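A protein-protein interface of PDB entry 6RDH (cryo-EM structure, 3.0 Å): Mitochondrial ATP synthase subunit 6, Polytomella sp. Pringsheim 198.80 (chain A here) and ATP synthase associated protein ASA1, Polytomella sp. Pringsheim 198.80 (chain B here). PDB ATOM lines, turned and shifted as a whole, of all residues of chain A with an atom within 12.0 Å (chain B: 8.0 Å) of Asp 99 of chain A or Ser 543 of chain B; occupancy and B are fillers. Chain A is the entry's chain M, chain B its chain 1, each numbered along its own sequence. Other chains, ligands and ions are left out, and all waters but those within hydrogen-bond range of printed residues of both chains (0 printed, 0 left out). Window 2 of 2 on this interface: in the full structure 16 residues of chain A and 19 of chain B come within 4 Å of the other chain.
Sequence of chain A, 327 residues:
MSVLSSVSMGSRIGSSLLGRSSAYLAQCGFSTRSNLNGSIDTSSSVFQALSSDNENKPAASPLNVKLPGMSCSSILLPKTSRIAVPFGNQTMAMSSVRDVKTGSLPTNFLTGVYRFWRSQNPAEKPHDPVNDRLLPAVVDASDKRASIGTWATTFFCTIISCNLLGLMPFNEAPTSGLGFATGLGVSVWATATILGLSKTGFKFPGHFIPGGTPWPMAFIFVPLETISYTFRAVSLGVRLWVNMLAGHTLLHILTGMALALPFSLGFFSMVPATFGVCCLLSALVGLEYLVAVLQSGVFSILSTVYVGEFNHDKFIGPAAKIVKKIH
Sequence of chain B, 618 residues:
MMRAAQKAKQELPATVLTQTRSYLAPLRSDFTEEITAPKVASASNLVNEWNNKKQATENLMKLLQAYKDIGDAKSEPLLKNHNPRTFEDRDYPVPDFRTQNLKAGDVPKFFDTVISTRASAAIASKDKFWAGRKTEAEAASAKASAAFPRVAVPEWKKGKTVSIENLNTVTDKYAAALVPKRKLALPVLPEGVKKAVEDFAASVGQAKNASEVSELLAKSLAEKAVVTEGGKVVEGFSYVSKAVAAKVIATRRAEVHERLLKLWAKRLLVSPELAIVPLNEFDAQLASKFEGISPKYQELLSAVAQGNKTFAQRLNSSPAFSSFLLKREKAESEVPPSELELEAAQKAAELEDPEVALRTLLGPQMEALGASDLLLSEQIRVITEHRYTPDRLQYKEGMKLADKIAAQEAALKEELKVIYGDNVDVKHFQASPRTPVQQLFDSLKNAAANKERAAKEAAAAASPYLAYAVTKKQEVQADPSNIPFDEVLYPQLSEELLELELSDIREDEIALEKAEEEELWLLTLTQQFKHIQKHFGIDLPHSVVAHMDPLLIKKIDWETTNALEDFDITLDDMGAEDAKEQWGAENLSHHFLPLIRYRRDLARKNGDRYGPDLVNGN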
ATOM      1  N   SER A  95     -15.281 -34.108 -27.275  1.00  0.00           N
ATOM      2  CA  SER A  95     -15.216 -33.598 -28.639  1.00  0.00           C
ATOM      3  C   SER A  95     -16.540 -32.960 -29.033  1.00  0.00           C
ATOM      4  O   SER A  95     -16.605 -31.761 -29.300  1.00  0.00           O
ATOM      5  CB  SER A  95     -14.855 -34.718 -29.620  1.00  0.00           C
ATOM      6  OG  SER A  95     -15.941 -35.608 -29.800  1.00  0.00           O
ATOM      7  N   SER A  96     -17.599 -33.765 -29.062  1.00  0.00           N
ATOM      8  CA  SER A  96     -18.930 -33.304 -29.439  1.00  0.00           C
ATOM      9  C   SER A  96     -19.831 -33.372 -28.210  1.00  0.00           C
ATOM     10  O   SER A  96     -20.558 -34.341 -28.001  1.00  0.00           O
ATOM     11  CB  SER A  96     -19.486 -34.143 -30.582  1.00  0.00           C
ATOM     12  OG  SER A  96     -20.901 -34.083 -30.608  1.00  0.00           O
ATOM     13  N   VAL A  97     -19.797 -32.315 -27.406  1.00  0.00           N
ATOM     14  CA  VAL A  97     -20.689 -32.242 -26.262  1.00  0.00           C
ATOM     15  C   VAL A  97     -21.975 -31.529 -26.660  1.00  0.00           C
ATOM     16  O   VAL A  97     -22.054 -30.849 -27.684  1.00  0.00           O
ATOM     17  CB  VAL A  97     -20.011 -31.557 -25.071  1.00  0.00           C
ATOM     18  CG1 VAL A  97     -18.667 -32.164 -24.857  1.00  0.00           C
ATOM     19  CG2 VAL A  97     -19.886 -30.092 -25.312  1.00  0.00           C
ATOM     20  N   ARG A  98     -23.003 -31.710 -25.844  1.00  0.00           N
ATOM     21  CA  ARG A  98     -24.303 -31.172 -26.183  1.00  0.00           C
ATOM     22  C   ARG A  98     -24.360 -29.685 -25.884  1.00  0.00           C
ATOM     23  O   ARG A  98     -23.611 -29.158 -25.065  1.00  0.00           O
ATOM     24  CB  ARG A  98     -25.398 -31.904 -25.420  1.00  0.00           C
ATOM     25  CG  ARG A  98     -25.253 -31.833 -23.928  1.00  0.00           C
ATOM     26  CD  ARG A  98     -25.975 -32.981 -23.279  1.00  0.00           C
ATOM     27  NE  ARG A  98     -25.473 -34.261 -23.759  1.00  0.00           N
ATOM     28  CZ  ARG A  98     -25.993 -35.430 -23.420  1.00  0.00           C
ATOM     29  NH1 ARG A  98     -27.026 -35.472 -22.602  1.00  0.00           N
ATOM     30  NH2 ARG A  98     -25.484 -36.551 -23.899  1.00  0.00           N
ATOM     31  N   ASP A  99     -25.256 -29.008 -26.579  1.00  0.00           N
ATOM     32  CA  ASP A  99     -25.466 -27.585 -26.403  1.00  0.00           C
ATOM     33  C   ASP A  99     -26.547 -27.387 -25.359  1.00  0.00           C
ATOM     34  O   ASP A  99     -27.549 -28.103 -25.347  1.00  0.00           O
ATOM     35  CB  ASP A  99     -25.870 -26.931 -27.721  1.00  0.00           C
ATOM     36  CG  ASP A  99     -25.589 -25.455 -27.751  1.00  0.00           C
ATOM     37  OD1 ASP A  99     -25.300 -24.877 -26.693  1.00  0.00           O
ATOM     38  OD2 ASP A  99     -25.645 -24.866 -28.842  1.00  0.00           O
ATOM     39  N   VAL A 100     -26.329 -26.434 -24.469  1.00  0.00           N
ATOM     40  CA  VAL A 100     -27.223 -26.197 -23.350  1.00  0.00           C
ATOM     41  C   VAL A 100     -27.845 -24.824 -23.518  1.00  0.00           C
ATOM     42  O   VAL A 100     -27.150 -23.860 -23.843  1.00  0.00           O
ATOM     43  CB  VAL A 100     -26.478 -26.290 -22.007  1.00  0.00           C
ATOM     44  CG1 VAL A 100     -27.450 -26.249 -20.867  1.00  0.00           C
ATOM     45  CG2 VAL A 100     -25.657 -27.537 -21.951  1.00  0.00           C
ATOM     46  N   LYS A 101     -29.148 -24.741 -23.315  1.00  0.00           N
ATOM     47  CA  LYS A 101     -29.806 -23.453 -23.227  1.00  0.00           C
ATOM     48  C   LYS A 101     -29.406 -22.764 -21.938  1.00  0.00           C
ATOM     49  O   LYS A 101     -29.288 -23.403 -20.893  1.00  0.00           O
ATOM     50  CB  LYS A 101     -31.312 -23.650 -23.263  1.00  0.00           C
ATOM     51  CG  LYS A 101     -32.118 -22.415 -23.407  1.00  0.00           C
ATOM     52  CD  LYS A 101     -33.552 -22.798 -23.592  1.00  0.00           C
ATOM     53  CE  LYS A 101     -34.212 -23.048 -22.277  1.00  0.00           C
ATOM     54  NZ  LYS A 101     -34.534 -21.766 -21.611  1.00  0.00           N
ATOM     55  N   THR A 102     -29.171 -21.462 -22.005  1.00  0.00           N
ATOM     56  CA  THR A 102     -28.946 -20.721 -20.780  1.00  0.00           C
ATOM     57  C   THR A 102     -30.274 -20.483 -20.091  1.00  0.00           C
ATOM     58  O   THR A 102     -31.291 -20.236 -20.734  1.00  0.00           O
ATOM     59  CB  THR A 102     -28.270 -19.383 -21.039  1.00  0.00           C
ATOM     60  OG1 THR A 102     -28.944 -18.720 -22.101  1.00  0.00           O
ATOM     61  CG2 THR A 102     -26.836 -19.572 -21.416  1.00  0.00           C
ATOM     62  N   GLY A 103     -30.260 -20.567 -18.769  1.00  0.00           N
ATOM     63  CA  GLY A 103     -31.476 -20.334 -18.028  1.00  0.00           C
ATOM     64  C   GLY A 103     -32.465 -21.461 -18.117  1.00  0.00           C
ATOM     65  O   GLY A 103     -33.670 -21.220 -18.071  1.00  0.00           O
ATOM     66  N   SER A 104     -31.986 -22.689 -18.273  1.00  0.00           N
ATOM     67  CA  SER A 104     -32.847 -23.852 -18.175  1.00  0.00           C
ATOM     68  C   SER A 104     -33.285 -24.046 -16.738  1.00  0.00           C
ATOM     69  O   SER A 104     -32.623 -23.605 -15.806  1.00  0.00           O
ATOM     70  CB  SER A 104     -32.120 -25.096 -18.650  1.00  0.00           C
ATOM     71  OG  SER A 104     -31.945 -25.078 -20.046  1.00  0.00           O
ATOM     72  N   LEU A 105     -34.408 -24.701 -16.561  1.00  0.00           N
ATOM     73  CA  LEU A 105     -34.888 -25.018 -15.222  1.00  0.00           C
ATOM     74  C   LEU A 105     -34.009 -26.001 -14.439  1.00  0.00           C
ATOM     75  O   LEU A 105     -33.861 -25.803 -13.226  1.00  0.00           O
ATOM     76  CB  LEU A 105     -36.330 -25.520 -15.300  1.00  0.00           C
ATOM     77  CG  LEU A 105     -37.090 -25.821 -14.017  1.00  0.00           C
ATOM     78  CD1 LEU A 105     -38.453 -25.232 -14.112  1.00  0.00           C
ATOM     79  CD2 LEU A 105     -37.209 -27.307 -13.836  1.00  0.00           C
ATOM     80  N   PRO A 106     -33.413 -27.055 -15.029  1.00  0.00           N
ATOM     81  CA  PRO A 106     -32.451 -27.835 -14.240  1.00  0.00           C
ATOM     82  C   PRO A 106     -31.192 -27.081 -13.885  1.00  0.00           C
ATOM     83  O   PRO A 106     -30.640 -27.309 -12.807  1.00  0.00           O
ATOM     84  CB  PRO A 106     -32.144 -29.025 -15.149  1.00  0.00           C
ATOM     85  CG  PRO A 106     -33.316 -29.170 -15.928  1.00  0.00           C
ATOM     86  CD  PRO A 106     -33.738 -27.807 -16.256  1.00  0.00           C
ATOM     87  N   THR A 107     -30.735 -26.176 -14.743  1.00  0.00           N
ATOM     88  CA  THR A 107     -29.556 -25.384 -14.428  1.00  0.00           C
ATOM     89  C   THR A 107     -29.843 -24.400 -13.306  1.00  0.00           C
ATOM     90  O   THR A 107     -29.022 -24.235 -12.402  1.00  0.00           O
ATOM     91  CB  THR A 107     -29.078 -24.666 -15.684  1.00  0.00           C
ATOM     92  OG1 THR A 107     -28.914 -25.619 -16.735  1.00  0.00           O
ATOM     93  CG2 THR A 107     -27.766 -24.031 -15.452  1.00  0.00           C
ATOM     94  N   ASP B 539     -33.063 -17.868 -24.059  1.00  0.00           N
ATOM     95  CA  ASP B 539     -32.850 -18.909 -25.052  1.00  0.00           C
ATOM     96  C   ASP B 539     -31.451 -18.944 -25.639  1.00  0.00           C
ATOM     97  O   ASP B 539     -31.267 -19.593 -26.662  1.00  0.00           O
ATOM     98  CB  ASP B 539     -33.871 -18.805 -26.198  1.00  0.00           C
ATOM     99  CG  ASP B 539     -34.031 -17.391 -26.754  1.00  0.00           C
ATOM    100  OD1 ASP B 539     -33.040 -16.655 -26.894  1.00  0.00           O
ATOM    101  OD2 ASP B 539     -35.172 -17.011 -27.080  1.00  0.00           O
ATOM    102  N   LEU B 540     -30.482 -18.275 -25.062  1.00  0.00           N
ATOM    103  CA  LEU B 540     -29.158 -18.256 -25.664  1.00  0.00           C
ATOM    104  C   LEU B 540     -28.470 -19.583 -25.413  1.00  0.00           C
ATOM    105  O   LEU B 540     -28.408 -20.022 -24.270  1.00  0.00           O
ATOM    106  CB  LEU B 540     -28.324 -17.137 -25.074  1.00  0.00           C
ATOM    107  CG  LEU B 540     -26.970 -16.719 -25.629  1.00  0.00           C
ATOM    108  CD1 LEU B 540     -27.050 -16.420 -27.078  1.00  0.00           C
ATOM    109  CD2 LEU B 540     -26.542 -15.500 -24.907  1.00  0.00           C
ATOM    110  N   PRO B 541     -27.980 -20.265 -26.435  1.00  0.00           N
ATOM    111  CA  PRO B 541     -27.234 -21.489 -26.186  1.00  0.00           C
ATOM    112  C   PRO B 541     -25.849 -21.197 -25.654  1.00  0.00           C
ATOM    113  O   PRO B 541     -25.327 -20.092 -25.754  1.00  0.00           O
ATOM    114  CB  PRO B 541     -27.178 -22.165 -27.553  1.00  0.00           C
ATOM    115  CG  PRO B 541     -27.514 -21.188 -28.480  1.00  0.00           C
ATOM    116  CD  PRO B 541     -28.311 -20.136 -27.853  1.00  0.00           C
ATOM    117  N   HIS B 542     -25.262 -22.217 -25.048  1.00  0.00           N
ATOM    118  CA  HIS B 542     -23.924 -22.073 -24.520  1.00  0.00           C
ATOM    119  C   HIS B 542     -22.883 -22.026 -25.617  1.00  0.00           C
ATOM    120  O   HIS B 542     -21.795 -21.491 -25.395  1.00  0.00           O
ATOM    121  CB  HIS B 542     -23.617 -23.223 -23.578  1.00  0.00           C
ATOM    122  CG  HIS B 542     -23.969 -22.956 -22.151  1.00  0.00           C
ATOM    123  ND1 HIS B 542     -25.256 -22.737 -21.731  1.00  0.00           N
ATOM    124  CD2 HIS B 542     -23.197 -22.893 -21.046  1.00  0.00           C
ATOM    125  CE1 HIS B 542     -25.264 -22.548 -20.426  1.00  0.00           C
ATOM    126  NE2 HIS B 542     -24.027 -22.635 -19.987  1.00  0.00           N
ATOM    127  N   SER B 543     -23.187 -22.576 -26.788  1.00  0.00           N
ATOM    128  CA  SER B 543     -22.226 -22.553 -27.880  1.00  0.00           C
ATOM    129  C   SER B 543     -22.071 -21.164 -28.450  1.00  0.00           C
ATOM    130  O   SER B 543     -20.969 -20.778 -28.833  1.00  0.00           O
ATOM    131  CB  SER B 543     -22.659 -23.506 -28.975  1.00  0.00           C
ATOM    132  OG  SER B 543     -23.984 -23.231 -29.358  1.00  0.00           O
ATOM    133  N   VAL B 544     -23.153 -20.392 -28.489  1.00  0.00           N
ATOM    134  CA  VAL B 544     -23.077 -19.022 -28.968  1.00  0.00           C
ATOM    135  C   VAL B 544     -22.357 -18.144 -27.962  1.00  0.00           C
ATOM    136  O   VAL B 544     -21.628 -17.227 -28.343  1.00  0.00           O
ATOM    137  CB  VAL B 544     -24.495 -18.539 -29.294  1.00  0.00           C
ATOM    138  CG1 VAL B 544     -24.496 -17.154 -29.771  1.00  0.00           C
ATOM    139  CG2 VAL B 544     -25.032 -19.378 -30.388  1.00  0.00           C
ATOM    140  N   VAL B 545     -22.494 -18.439 -26.672  1.00  0.00           N
ATOM    141  CA  VAL B 545     -21.743 -17.726 -25.641  1.00  0.00           C
ATOM    142  C   VAL B 545     -20.258 -18.034 -25.752  1.00  0.00           C
ATOM    143  O   VAL B 545     -19.414 -17.138 -25.683  1.00  0.00           O
ATOM    144  CB  VAL B 545     -22.290 -18.093 -24.254  1.00  0.00           C
ATOM    145  CG1 VAL B 545     -21.327 -17.731 -23.176  1.00  0.00           C
ATOM    146  CG2 VAL B 545     -23.575 -17.412 -24.015  1.00  0.00           C
ATOM    147  N   ALA B 546     -19.916 -19.304 -25.944  1.00  0.00           N
ATOM    148  CA  ALA B 546     -18.517 -19.681 -26.075  1.00  0.00           C
ATOM    149  C   ALA B 546     -17.932 -19.283 -27.416  1.00  0.00           C
ATOM    150  O   ALA B 546     -16.711 -19.278 -27.568  1.00  0.00           O
ATOM    151  CB  ALA B 546     -18.362 -21.182 -25.872  1.00  0.00           C
ATOM    152  N   HIS B 547     -18.773 -18.984 -28.398  1.00  0.00           N
ATOM    153  CA  HIS B 547     -18.289 -18.451 -29.659  1.00  0.00           C
ATOM    154  C   HIS B 547     -18.028 -16.963 -29.546  1.00  0.00           C
ATOM    155  O   HIS B 547     -16.950 -16.489 -29.904  1.00  0.00           O
ATOM    156  CB  HIS B 547     -19.302 -18.731 -30.760  1.00  0.00           C
ATOM    157  CG  HIS B 547     -18.915 -18.177 -32.088  1.00  0.00           C
ATOM    158  ND1 HIS B 547     -19.494 -17.050 -32.619  1.00  0.00           N
ATOM    159  CD2 HIS B 547     -18.003 -18.595 -32.993  1.00  0.00           C
ATOM    160  CE1 HIS B 547     -18.957 -16.794 -33.796  1.00  0.00           C
ATOM    161  NE2 HIS B 547     -18.048 -17.717 -34.045  1.00  0.00           N
ATOM    162  N   MET B 548     -19.008 -16.222 -29.033  1.00  0.00           N
ATOM    163  CA  MET B 548     -18.897 -14.779 -28.888  1.00  0.00           C
ATOM    164  C   MET B 548     -17.804 -14.396 -27.905  1.00  0.00           C
ATOM    165  O   MET B 548     -17.068 -13.435 -28.133  1.00  0.00           O
ATOM    166  CB  MET B 548     -20.225 -14.213 -28.414  1.00  0.00           C
ATOM    167  CG  MET B 548     -21.048 -13.597 -29.480  1.00  0.00           C
ATOM    168  SD  MET B 548     -22.423 -12.745 -28.745  1.00  0.00           S
ATOM    169  CE  MET B 548     -23.288 -14.151 -28.133  1.00  0.00           C
ATOM    170  N   ASP B 549     -17.678 -15.127 -26.811  1.00  0.00           N
ATOM    171  CA  ASP B 549     -16.734 -14.791 -25.751  1.00  0.00           C
ATOM    172  C   ASP B 549     -15.921 -16.024 -25.399  1.00  0.00           C
ATOM    173  O   ASP B 549     -16.254 -16.748 -24.456  1.00  0.00           O
ATOM    174  CB  ASP B 549     -17.467 -14.249 -24.532  1.00  0.00           C
ATOM    175  CG  ASP B 549     -16.705 -13.162 -23.858  1.00  0.00           C
ATOM    176  OD1 ASP B 549     -15.581 -12.900 -24.306  1.00  0.00           O
ATOM    177  OD2 ASP B 549     -17.229 -12.543 -22.915  1.00  0.00           O
ATOM    178  N   ILE B 553     -15.071 -17.816 -21.315  1.00  0.00           N
ATOM    179  CA  ILE B 553     -15.334 -19.230 -21.092  1.00  0.00           C
ATOM    180  C   ILE B 553     -14.057 -19.962 -20.722  1.00  0.00           C
ATOM    181  O   ILE B 553     -14.074 -20.850 -19.869  1.00  0.00           O
ATOM    182  CB  ILE B 553     -16.018 -19.800 -22.346  1.00  0.00           C
ATOM    183  CG1 ILE B 553     -17.443 -19.265 -22.451  1.00  0.00           C
ATOM    184  CG2 ILE B 553     -16.018 -21.281 -22.376  1.00  0.00           C
ATOM    185  CD1 ILE B 553     -18.255 -19.365 -21.207  1.00  0.00           C
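The backbone carbonyl oxygen (O) of Val 100 of chain A is in hydrogen-bond range of the backbone NH (N) of His 542 of chain B, 2.8 Å away. OG1 of Thr 102 of chain A lies within hydrogen-bond range of O of Leu 540 of chain B (2.6 Å). OD1 of Asp 99 of chain A sits at hydrogen-bond distance from N of Ser 543 of chain B, at 3.1 Å. The side-chain carboxylate of Asp 99 of chain A is in hydrogen-bond range of the backbone NH of His 542 of chain B, 3.1 Å away.
O of Lys 101 of chain A lies within hydrogen-bond range of OG of Ser 104 of chain A (3.3 Å).
Among the printed residues, pairs that only touch across the chains: Val 100 of chain A with Pro 541 of chain B, Asp 99 of chain A with Pro 541 of chain B, Thr 102 of chain A with His 542 of chain B, Lys 101 of chain A with Leu 540 of chain B and Lys 101 of chain A with Asp 539 of chain B.
Asp 99 of chain A touches just these residues of chain B: Pro 541, His 542 and Ser 543. Ser 543 of chain B touches just one residue of chain A: Asp 99 (2.4 Å). Pro 541 of chain B touches two residues of chain A. Printed residues of chain A within 4 Å of His 542 of chain B: Asp 99, Val 100 and Thr 102. No residue of chain A comes within 4 Å of Val 544 of chain B. No residue of chain A comes within 4 Å of Val 545 of chain B. No residue of chain A comes within 4 Å of His 547 of chain B. Of the printed residues of chain B, Lys 101 of chain A touches Asp 539 and Leu 540. Of the printed residues of chain B, Val 100 of chain A touches Pro 541 and His 542. The nearest residue of chain B that does not touch Asp 99 of chain A is Val 544 of chain B (5.1 Å).
Printed residues of chain B that touch a printed residue of chain A: Asp 539, Leu 540, Pro 541, His 542 and Ser 543. Along chain B the printed residues that touch a printed residue of chain A span positions 539 to 543. Among the printed residues, 9 pairs touch across the chains. Among the printed residues, no Asp or Glu carboxylate lies within 4 Å of a Lys or Arg side-chain nitrogen of the other chain.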
